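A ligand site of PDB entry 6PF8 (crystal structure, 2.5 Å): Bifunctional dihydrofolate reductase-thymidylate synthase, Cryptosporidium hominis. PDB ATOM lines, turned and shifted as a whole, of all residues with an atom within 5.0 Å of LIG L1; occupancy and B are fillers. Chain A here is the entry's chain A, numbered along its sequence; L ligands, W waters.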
ATOM      1  N   ARG A 257      11.071  13.028  26.676  1.00  0.00           N
ATOM      2  CA  ARG A 257       9.717  13.507  26.398  1.00  0.00           C
ATOM      3  C   ARG A 257       9.415  13.534  24.898  1.00  0.00           C
ATOM      4  O   ARG A 257       8.271  13.316  24.487  1.00  0.00           O
ATOM      5  CB  ARG A 257       9.531  14.894  27.020  1.00  0.00           C
ATOM      6  CG  ARG A 257      10.551  15.912  26.543  1.00  0.00           C
ATOM      7  CD  ARG A 257      10.357  17.266  27.207  1.00  0.00           C
ATOM      8  NE  ARG A 257      10.975  18.334  26.439  1.00  0.00           N
ATOM      9  CZ  ARG A 257      10.396  18.943  25.409  1.00  0.00           C
ATOM     10  NH1 ARG A 257       9.165  18.581  25.049  1.00  0.00           N
ATOM     11  NH2 ARG A 257      11.016  19.908  24.754  1.00  0.00           N
ATOM     12  N   LYS A 284      31.371  24.639  11.893  1.00  0.00           N
ATOM     13  CA  LYS A 284      30.004  24.688  11.381  1.00  0.00           C
ATOM     14  C   LYS A 284      29.579  26.142  11.347  1.00  0.00           C
ATOM     15  O   LYS A 284      29.850  26.894  12.292  1.00  0.00           O
ATOM     16  CB  LYS A 284      29.051  23.864  12.248  1.00  0.00           C
ATOM     17  CG  LYS A 284      27.600  23.920  11.808  1.00  0.00           C
ATOM     18  CD  LYS A 284      26.693  23.243  12.822  1.00  0.00           C
ATOM     19  CE  LYS A 284      26.591  24.054  14.104  1.00  0.00           C
ATOM     20  NZ  LYS A 284      25.534  23.521  15.013  1.00  0.00           N
ATOM     21  N   LYS A 285      28.926  26.547  10.265  1.00  0.00           N
ATOM     22  CA  LYS A 285      28.412  27.915  10.179  1.00  0.00           C
ATOM     23  C   LYS A 285      27.233  28.070  11.136  1.00  0.00           C
ATOM     24  O   LYS A 285      26.219  27.374  10.994  1.00  0.00           O
ATOM     25  CB  LYS A 285      28.001  28.255   8.760  1.00  0.00           C
ATOM     26  CG  LYS A 285      27.557  29.692   8.574  1.00  0.00           C
ATOM     27  CD  LYS A 285      27.206  29.983   7.123  1.00  0.00           C
ATOM     28  CE  LYS A 285      26.712  31.413   6.939  1.00  0.00           C
ATOM     29  NZ  LYS A 285      26.389  31.708   5.510  1.00  0.00           N
ATOM     30  N   ALA A 287      24.221  30.298  12.959  1.00  0.00           N
ATOM     31  CA  ALA A 287      23.294  31.394  12.648  1.00  0.00           C
ATOM     32  C   ALA A 287      23.408  32.455  13.735  1.00  0.00           C
ATOM     33  O   ALA A 287      22.606  32.526  14.676  1.00  0.00           O
ATOM     34  CB  ALA A 287      21.879  30.871  12.510  1.00  0.00           C
ATOM     35  N   SER A 290      20.241  34.858  14.363  1.00  0.00           N
ATOM     36  CA  SER A 290      19.175  34.299  15.177  1.00  0.00           C
ATOM     37  C   SER A 290      19.550  34.281  16.650  1.00  0.00           C
ATOM     38  O   SER A 290      18.703  34.495  17.517  1.00  0.00           O
ATOM     39  CB  SER A 290      18.835  32.881  14.696  1.00  0.00           C
ATOM     40  OG  SER A 290      18.434  32.889  13.337  1.00  0.00           O
ATOM     41  N   GLU A 294      17.398  36.345  19.488  1.00  0.00           N
ATOM     42  CA  GLU A 294      16.817  35.692  20.651  1.00  0.00           C
ATOM     43  C   GLU A 294      17.280  36.344  21.944  1.00  0.00           C
ATOM     44  O   GLU A 294      16.506  36.481  22.894  1.00  0.00           O
ATOM     45  CB  GLU A 294      17.168  34.200  20.650  1.00  0.00           C
ATOM     46  CG  GLU A 294      16.533  33.414  21.795  1.00  0.00           C
ATOM     47  CD  GLU A 294      17.187  32.059  22.017  1.00  0.00           C
ATOM     48  OE1 GLU A 294      18.429  31.977  21.913  1.00  0.00           O
ATOM     49  OE2 GLU A 294      16.464  31.085  22.298  1.00  0.00           O
ATOM     50  N   ILE A 315      13.288  29.632  15.747  1.00  0.00           N
ATOM     51  CA  ILE A 315      13.812  28.612  16.640  1.00  0.00           C
ATOM     52  C   ILE A 315      12.788  28.233  17.705  1.00  0.00           C
ATOM     53  O   ILE A 315      12.812  27.108  18.228  1.00  0.00           O
ATOM     54  CB  ILE A 315      15.147  29.069  17.265  1.00  0.00           C
ATOM     55  CG1 ILE A 315      14.943  30.323  18.106  1.00  0.00           C
ATOM     56  CG2 ILE A 315      16.179  29.316  16.171  1.00  0.00           C
ATOM     57  CD1 ILE A 315      16.189  30.776  18.834  1.00  0.00           C
ATOM     58  N   TRP A 316      11.881  29.140  18.049  1.00  0.00           N
ATOM     59  CA  TRP A 316      10.860  28.888  19.050  1.00  0.00           C
ATOM     60  C   TRP A 316       9.511  28.519  18.447  1.00  0.00           C
ATOM     61  O   TRP A 316       8.496  28.557  19.145  1.00  0.00           O
ATOM     62  CB  TRP A 316      10.703  30.109  19.971  1.00  0.00           C
ATOM     63  CG  TRP A 316      11.760  30.184  21.036  1.00  0.00           C
ATOM     64  CD1 TRP A 316      12.902  30.921  20.987  1.00  0.00           C
ATOM     65  CD2 TRP A 316      11.771  29.490  22.281  1.00  0.00           C
ATOM     66  NE1 TRP A 316      13.627  30.731  22.141  1.00  0.00           N
ATOM     67  CE2 TRP A 316      12.950  29.854  22.956  1.00  0.00           C
ATOM     68  CE3 TRP A 316      10.889  28.590  22.906  1.00  0.00           C
ATOM     69  CZ2 TRP A 316      13.283  29.359  24.213  1.00  0.00           C
ATOM     70  CZ3 TRP A 316      11.218  28.104  24.153  1.00  0.00           C
ATOM     71  CH2 TRP A 316      12.403  28.486  24.804  1.00  0.00           C
ATOM     72  N   ASN A 319       8.089  24.745  19.866  1.00  0.00           N
ATOM     73  CA  ASN A 319       7.530  24.751  21.215  1.00  0.00           C
ATOM     74  C   ASN A 319       6.449  25.801  21.395  1.00  0.00           C
ATOM     75  O   ASN A 319       6.055  26.081  22.528  1.00  0.00           O
ATOM     76  CB  ASN A 319       8.648  24.950  22.239  1.00  0.00           C
ATOM     77  CG  ASN A 319       9.709  23.869  22.165  1.00  0.00           C
ATOM     78  OD1 ASN A 319      10.835  24.113  21.754  1.00  0.00           O
ATOM     79  ND2 ASN A 319       9.346  22.647  22.545  1.00  0.00           N
ATOM     80  N   LEU A 399       8.178  25.609  27.999  1.00  0.00           N
ATOM     81  CA  LEU A 399       9.344  24.761  28.228  1.00  0.00           C
ATOM     82  C   LEU A 399      10.109  25.290  29.440  1.00  0.00           C
ATOM     83  O   LEU A 399      10.368  26.504  29.528  1.00  0.00           O
ATOM     84  CB  LEU A 399      10.235  24.726  26.982  1.00  0.00           C
ATOM     85  CG  LEU A 399      11.247  23.590  26.906  1.00  0.00           C
ATOM     86  CD1 LEU A 399      10.549  22.239  26.946  1.00  0.00           C
ATOM     87  CD2 LEU A 399      12.084  23.722  25.637  1.00  0.00           C
ATOM     88  N   ASP A 426      21.140  20.203  24.438  1.00  0.00           N
ATOM     89  CA  ASP A 426      21.102  19.662  23.086  1.00  0.00           C
ATOM     90  C   ASP A 426      22.385  20.067  22.376  1.00  0.00           C
ATOM     91  O   ASP A 426      22.519  21.188  21.892  1.00  0.00           O
ATOM     92  CB  ASP A 426      19.863  20.184  22.357  1.00  0.00           C
ATOM     93  CG  ASP A 426      19.739  19.656  20.940  1.00  0.00           C
ATOM     94  OD1 ASP A 426      20.624  18.901  20.474  1.00  0.00           O
ATOM     95  OD2 ASP A 426      18.737  19.988  20.277  1.00  0.00           O
ATOM     96  N   LEU A 429      22.153  21.303  18.414  1.00  0.00           N
ATOM     97  CA  LEU A 429      21.520  22.575  18.067  1.00  0.00           C
ATOM     98  C   LEU A 429      21.617  23.614  19.169  1.00  0.00           C
ATOM     99  O   LEU A 429      22.011  24.751  18.907  1.00  0.00           O
ATOM    100  CB  LEU A 429      20.040  22.336  17.713  1.00  0.00           C
ATOM    101  CG  LEU A 429      19.765  21.531  16.447  1.00  0.00           C
ATOM    102  CD1 LEU A 429      18.278  21.354  16.244  1.00  0.00           C
ATOM    103  CD2 LEU A 429      20.399  22.218  15.247  1.00  0.00           C
ATOM    104  N   GLY A 430      21.258  23.244  20.402  1.00  0.00           N
ATOM    105  CA  GLY A 430      21.181  24.246  21.455  1.00  0.00           C
ATOM    106  C   GLY A 430      22.536  24.737  21.920  1.00  0.00           C
ATOM    107  O   GLY A 430      22.726  25.930  22.128  1.00  0.00           O
ATOM    108  N   PHE A 433      24.357  27.585  20.149  1.00  0.00           N
ATOM    109  CA  PHE A 433      23.638  28.821  20.431  1.00  0.00           C
ATOM    110  C   PHE A 433      23.949  29.335  21.830  1.00  0.00           C
ATOM    111  O   PHE A 433      24.228  30.522  22.013  1.00  0.00           O
ATOM    112  CB  PHE A 433      22.132  28.600  20.254  1.00  0.00           C
ATOM    113  CG  PHE A 433      21.645  28.844  18.856  1.00  0.00           C
ATOM    114  CD1 PHE A 433      22.270  28.265  17.765  1.00  0.00           C
ATOM    115  CD2 PHE A 433      20.541  29.655  18.631  1.00  0.00           C
ATOM    116  CE1 PHE A 433      21.824  28.490  16.481  1.00  0.00           C
ATOM    117  CE2 PHE A 433      20.086  29.884  17.343  1.00  0.00           C
ATOM    118  CZ  PHE A 433      20.725  29.299  16.272  1.00  0.00           C
ATOM    119  N   TYR A 466      20.964  13.966  20.196  1.00  0.00           N
ATOM    120  CA  TYR A 466      19.804  13.300  19.623  1.00  0.00           C
ATOM    121  C   TYR A 466      20.240  12.361  18.502  1.00  0.00           C
ATOM    122  O   TYR A 466      21.121  12.681  17.702  1.00  0.00           O
ATOM    123  CB  TYR A 466      18.807  14.335  19.093  1.00  0.00           C
ATOM    124  CG  TYR A 466      18.029  15.022  20.192  1.00  0.00           C
ATOM    125  CD1 TYR A 466      18.428  16.247  20.710  1.00  0.00           C
ATOM    126  CD2 TYR A 466      16.898  14.428  20.739  1.00  0.00           C
ATOM    127  CE1 TYR A 466      17.720  16.862  21.725  1.00  0.00           C
ATOM    128  CE2 TYR A 466      16.184  15.030  21.755  1.00  0.00           C
ATOM    129  CZ  TYR A 466      16.596  16.254  22.239  1.00  0.00           C
ATOM    130  OH  TYR A 466      15.882  16.856  23.255  1.00  0.00           O
ATOM    131  N   THR A 514      27.334  24.927   6.375  1.00  0.00           N
ATOM    132  CA  THR A 514      26.252  24.669   7.314  1.00  0.00           C
ATOM    133  C   THR A 514      25.918  23.179   7.362  1.00  0.00           C
ATOM    134  O   THR A 514      26.101  22.446   6.386  1.00  0.00           O
ATOM    135  CB  THR A 514      25.011  25.487   6.912  1.00  0.00           C
ATOM    136  OG1 THR A 514      25.354  26.879   6.873  1.00  0.00           O
ATOM    137  CG2 THR A 514      23.867  25.295   7.909  1.00  0.00           C
ATOM    138  N   ILE A 515      25.466  22.732   8.532  1.00  0.00           N
ATOM    139  CA  ILE A 515      25.055  21.347   8.752  1.00  0.00           C
ATOM    140  C   ILE A 515      23.619  21.367   9.280  1.00  0.00           C
ATOM    141  O   ILE A 515      23.371  21.865  10.386  1.00  0.00           O
ATOM    142  CB  ILE A 515      25.987  20.623   9.729  1.00  0.00           C
ATOM    143  CG1 ILE A 515      27.435  20.687   9.239  1.00  0.00           C
ATOM    144  CG2 ILE A 515      25.576  19.178   9.880  1.00  0.00           C
ATOM    145  CD1 ILE A 515      28.435  20.004  10.151  1.00  0.00           C
ATOM    146  N   MET A 517      20.260  20.198  10.932  1.00  0.00           N
ATOM    147  CA  MET A 517      19.844  19.274  11.983  1.00  0.00           C
ATOM    148  C   MET A 517      18.442  19.652  12.458  1.00  0.00           C
ATOM    149  O   MET A 517      18.188  20.818  12.754  1.00  0.00           O
ATOM    150  CB  MET A 517      20.827  19.291  13.167  1.00  0.00           C
ATOM    151  CG  MET A 517      22.107  18.516  12.924  1.00  0.00           C
ATOM    152  SD  MET A 517      23.296  18.689  14.276  1.00  0.00           S
ATOM    153  CE  MET A 517      24.000  20.297  13.896  1.00  0.00           C
ATOM    154  N   MET A 519      15.128  19.847  14.893  1.00  0.00           N
ATOM    155  CA  MET A 519      14.877  20.047  16.312  1.00  0.00           C
ATOM    156  C   MET A 519      13.844  19.053  16.824  1.00  0.00           C
ATOM    157  O   MET A 519      12.835  18.806  16.180  1.00  0.00           O
ATOM    158  CB  MET A 519      14.395  21.466  16.592  1.00  0.00           C
ATOM    159  CG  MET A 519      14.413  21.837  18.066  1.00  0.00           C
ATOM    160  SD  MET A 519      13.214  23.108  18.510  1.00  0.00           S
ATOM    161  CE  MET A 519      11.689  22.174  18.377  1.00  0.00           C
ATOM    162  N   ALA A 520      14.104  18.502  18.019  1.00  0.00           N
ATOM    163  CA  ALA A 520      13.183  17.582  18.660  1.00  0.00           C
ATOM    164  C   ALA A 520      12.153  18.379  19.460  1.00  0.00           C
ATOM    165  O   ALA A 520      12.508  19.119  20.386  1.00  0.00           O
ATOM    166  CB  ALA A 520      13.932  16.612  19.577  1.00  0.00           C
HETATM  167  N1  LIG L   1      14.363  22.186  22.142  1.00  0.00           N
HETATM  168  C1  LIG L   1      14.503  23.560  22.003  1.00  0.00           C
HETATM  169  O1  LIG L   1      17.841  23.855  20.776  1.00  0.00           O
HETATM  170  N2  LIG L   1      16.621  22.050  21.344  1.00  0.00           N
HETATM  171  C2  LIG L   1      15.622  24.216  21.560  1.00  0.00           C
HETATM  172  O2  LIG L   1      17.290  25.035  14.839  1.00  0.00           O
HETATM  173  N3  LIG L   1      13.540  24.498  22.287  1.00  0.00           N
HETATM  174  C3  LIG L   1      16.791  23.377  21.193  1.00  0.00           C
HETATM  175  O3  LIG L   1      17.284  27.923  13.516  1.00  0.00           O
HETATM  176  N4  LIG L   1      15.496  20.116  21.876  1.00  0.00           N
HETATM  177  C4  LIG L   1      15.421  21.491  21.810  1.00  0.00           C
HETATM  178  O4  LIG L   1      18.564  29.401  12.345  1.00  0.00           O
HETATM  179  C5  LIG L   1      15.331  25.616  21.569  1.00  0.00           C
HETATM  180  N5  LIG L   1      19.089  26.382  15.209  1.00  0.00           N
HETATM  181  C6  LIG L   1      14.050  25.759  22.024  1.00  0.00           C
HETATM  182  C7  LIG L   1      16.214  25.659  17.438  1.00  0.00           C
HETATM  183  C8  LIG L   1      17.509  26.015  16.998  1.00  0.00           C
HETATM  184  C9  LIG L   1      18.390  26.608  17.928  1.00  0.00           C
HETATM  185  C10 LIG L   1      17.994  26.848  19.258  1.00  0.00           C
HETATM  186  C11 LIG L   1      17.952  25.768  15.570  1.00  0.00           C
HETATM  187  C12 LIG L   1      19.795  26.343  13.955  1.00  0.00           C
HETATM  188  C13 LIG L   1      20.834  25.386  13.810  1.00  0.00           C
HETATM  189  C14 LIG L   1      21.568  25.282  12.616  1.00  0.00           C
HETATM  190  C15 LIG L   1      21.284  26.138  11.543  1.00  0.00           C
HETATM  191  C16 LIG L   1      20.262  27.093  11.670  1.00  0.00           C
HETATM  192  C17 LIG L   1      19.505  27.224  12.867  1.00  0.00           C
HETATM  193  C18 LIG L   1      18.428  28.292  12.879  1.00  0.00           C
HETATM  194  C19 LIG L   1      16.260  26.730  21.136  1.00  0.00           C
HETATM  195  C20 LIG L   1      16.699  26.492  19.698  1.00  0.00           C
HETATM  196  C21 LIG L   1      15.813  25.894  18.775  1.00  0.00           C
HETATM  197 CL1  LIG L   1      22.820  24.088  12.487  1.00  0.00          CL
HETATM  198  N1  LG2 L   2      17.767  22.916  24.795  1.00  0.00           N
HETATM  199  C1  LG2 L   2      19.053  23.336  25.023  1.00  0.00           C
HETATM  200  N2  LG2 L   2      19.334  24.650  25.111  1.00  0.00           N
HETATM  201  C2  LG2 L   2      18.380  25.583  24.978  1.00  0.00           C
HETATM  202  C3  LG2 L   2      17.045  25.171  24.734  1.00  0.00           C
HETATM  203  C4  LG2 L   2      16.786  23.854  24.646  1.00  0.00           C
HETATM  204  O1  LG2 L   2      19.995  22.583  25.159  1.00  0.00           O
HETATM  205  O2  LG2 L   2      18.648  26.769  25.067  1.00  0.00           O
HETATM  206  F1  LG2 L   2      16.047  26.078  24.593  1.00  0.00           F
HETATM  207  C5  LG2 L   2      17.319  21.508  24.664  1.00  0.00           C
HETATM  208  C6  LG2 L   2      17.884  20.503  25.709  1.00  0.00           C
HETATM  209  C7  LG2 L   2      16.927  19.315  25.496  1.00  0.00           C
HETATM  210  C8  LG2 L   2      15.614  19.981  25.038  1.00  0.00           C
HETATM  211  O3  LG2 L   2      17.408  18.462  24.452  1.00  0.00           O
HETATM  212  O4  LG2 L   2      15.902  21.404  24.939  1.00  0.00           O
HETATM  213  C9  LG2 L   2      14.441  19.682  25.982  1.00  0.00           C
HETATM  214  O5  LG2 L   2      14.728  20.169  27.290  1.00  0.00           O
HETATM  215  P1  LG2 L   2      14.074  19.151  28.361  1.00  0.00           P
HETATM  216  O6  LG2 L   2      13.539  17.831  27.599  1.00  0.00           O
HETATM  217  O7  LG2 L   2      15.093  18.765  29.364  1.00  0.00           O
HETATM  218  O8  LG2 L   2      12.855  19.869  29.100  1.00  0.00           O
HETATM  219  O   HOH W   1      11.981  20.619  22.374  1.00  0.00           O
HETATM  220  O   HOH W   2      14.858  26.440  13.633  1.00  0.00           O
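N of Asp 426 sits at hydrogen-bond distance from O1 of LG2 L2 (2.7 Å). An oxygen (O6) of LG2 L2 is in salt-bridge range of the guanidinium group (NE) of Arg 257, at 2.9 Å. O3 of LG2 L2 lies within hydrogen-bond range of OH of Tyr 466, 2.5 Å away. A nitrogen (N4) of LIG L1 is in hydrogen-bond range of the backbone carbonyl oxygen of Ala 520 (3.5 Å). N3 of LIG L1 sits at hydrogen-bond distance from OD1 of Asn 319 (2.8 Å). The side-chain carboxylate (OD2) of Asp 426 sits at hydrogen-bond distance from a nitrogen (N2) of LIG L1 (3.1 Å). N of Gly 430 sits close to O1 of LIG L1 (3.5 Å).
N4 of LIG L1 lies close to O4 of LG2 L2 (3.3 Å).
NZ of Lys 284 touches CL1 of LIG L1, 3.8 Å away. Ala 287 touches LIG L1 (CB to O4, 3.6 Å). Ser 290 touches LIG L1. CG2 of Ile 315 touches O3 of LIG L1, at 3.2 Å. Leu 399 touches LIG L1. CD2 of Leu 429 touches C13 of LIG L1 (3.5 Å). Phe 433 touches LIG L1. Tyr 466 touches LIG L1 (OH to N4, 3.6 Å). Ile 515 touches LIG L1. SD of Met 519 touches C1 of LIG L1, at 3.8 Å. Hydrophobic or aromatic side chains within 4 Å of LIG L1: Ala 287, Ile 315, Leu 399, Leu 429, Phe 433, Tyr 466 and Met 519.
Water W1 lies within hydrogen-bond range of O of Ala 520 (2.5 Å), NH2 of Arg 257 (2.7 Å), N1 of LIG L1 (2.9 Å) and ND2 of Asn 319 (3.3 Å).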
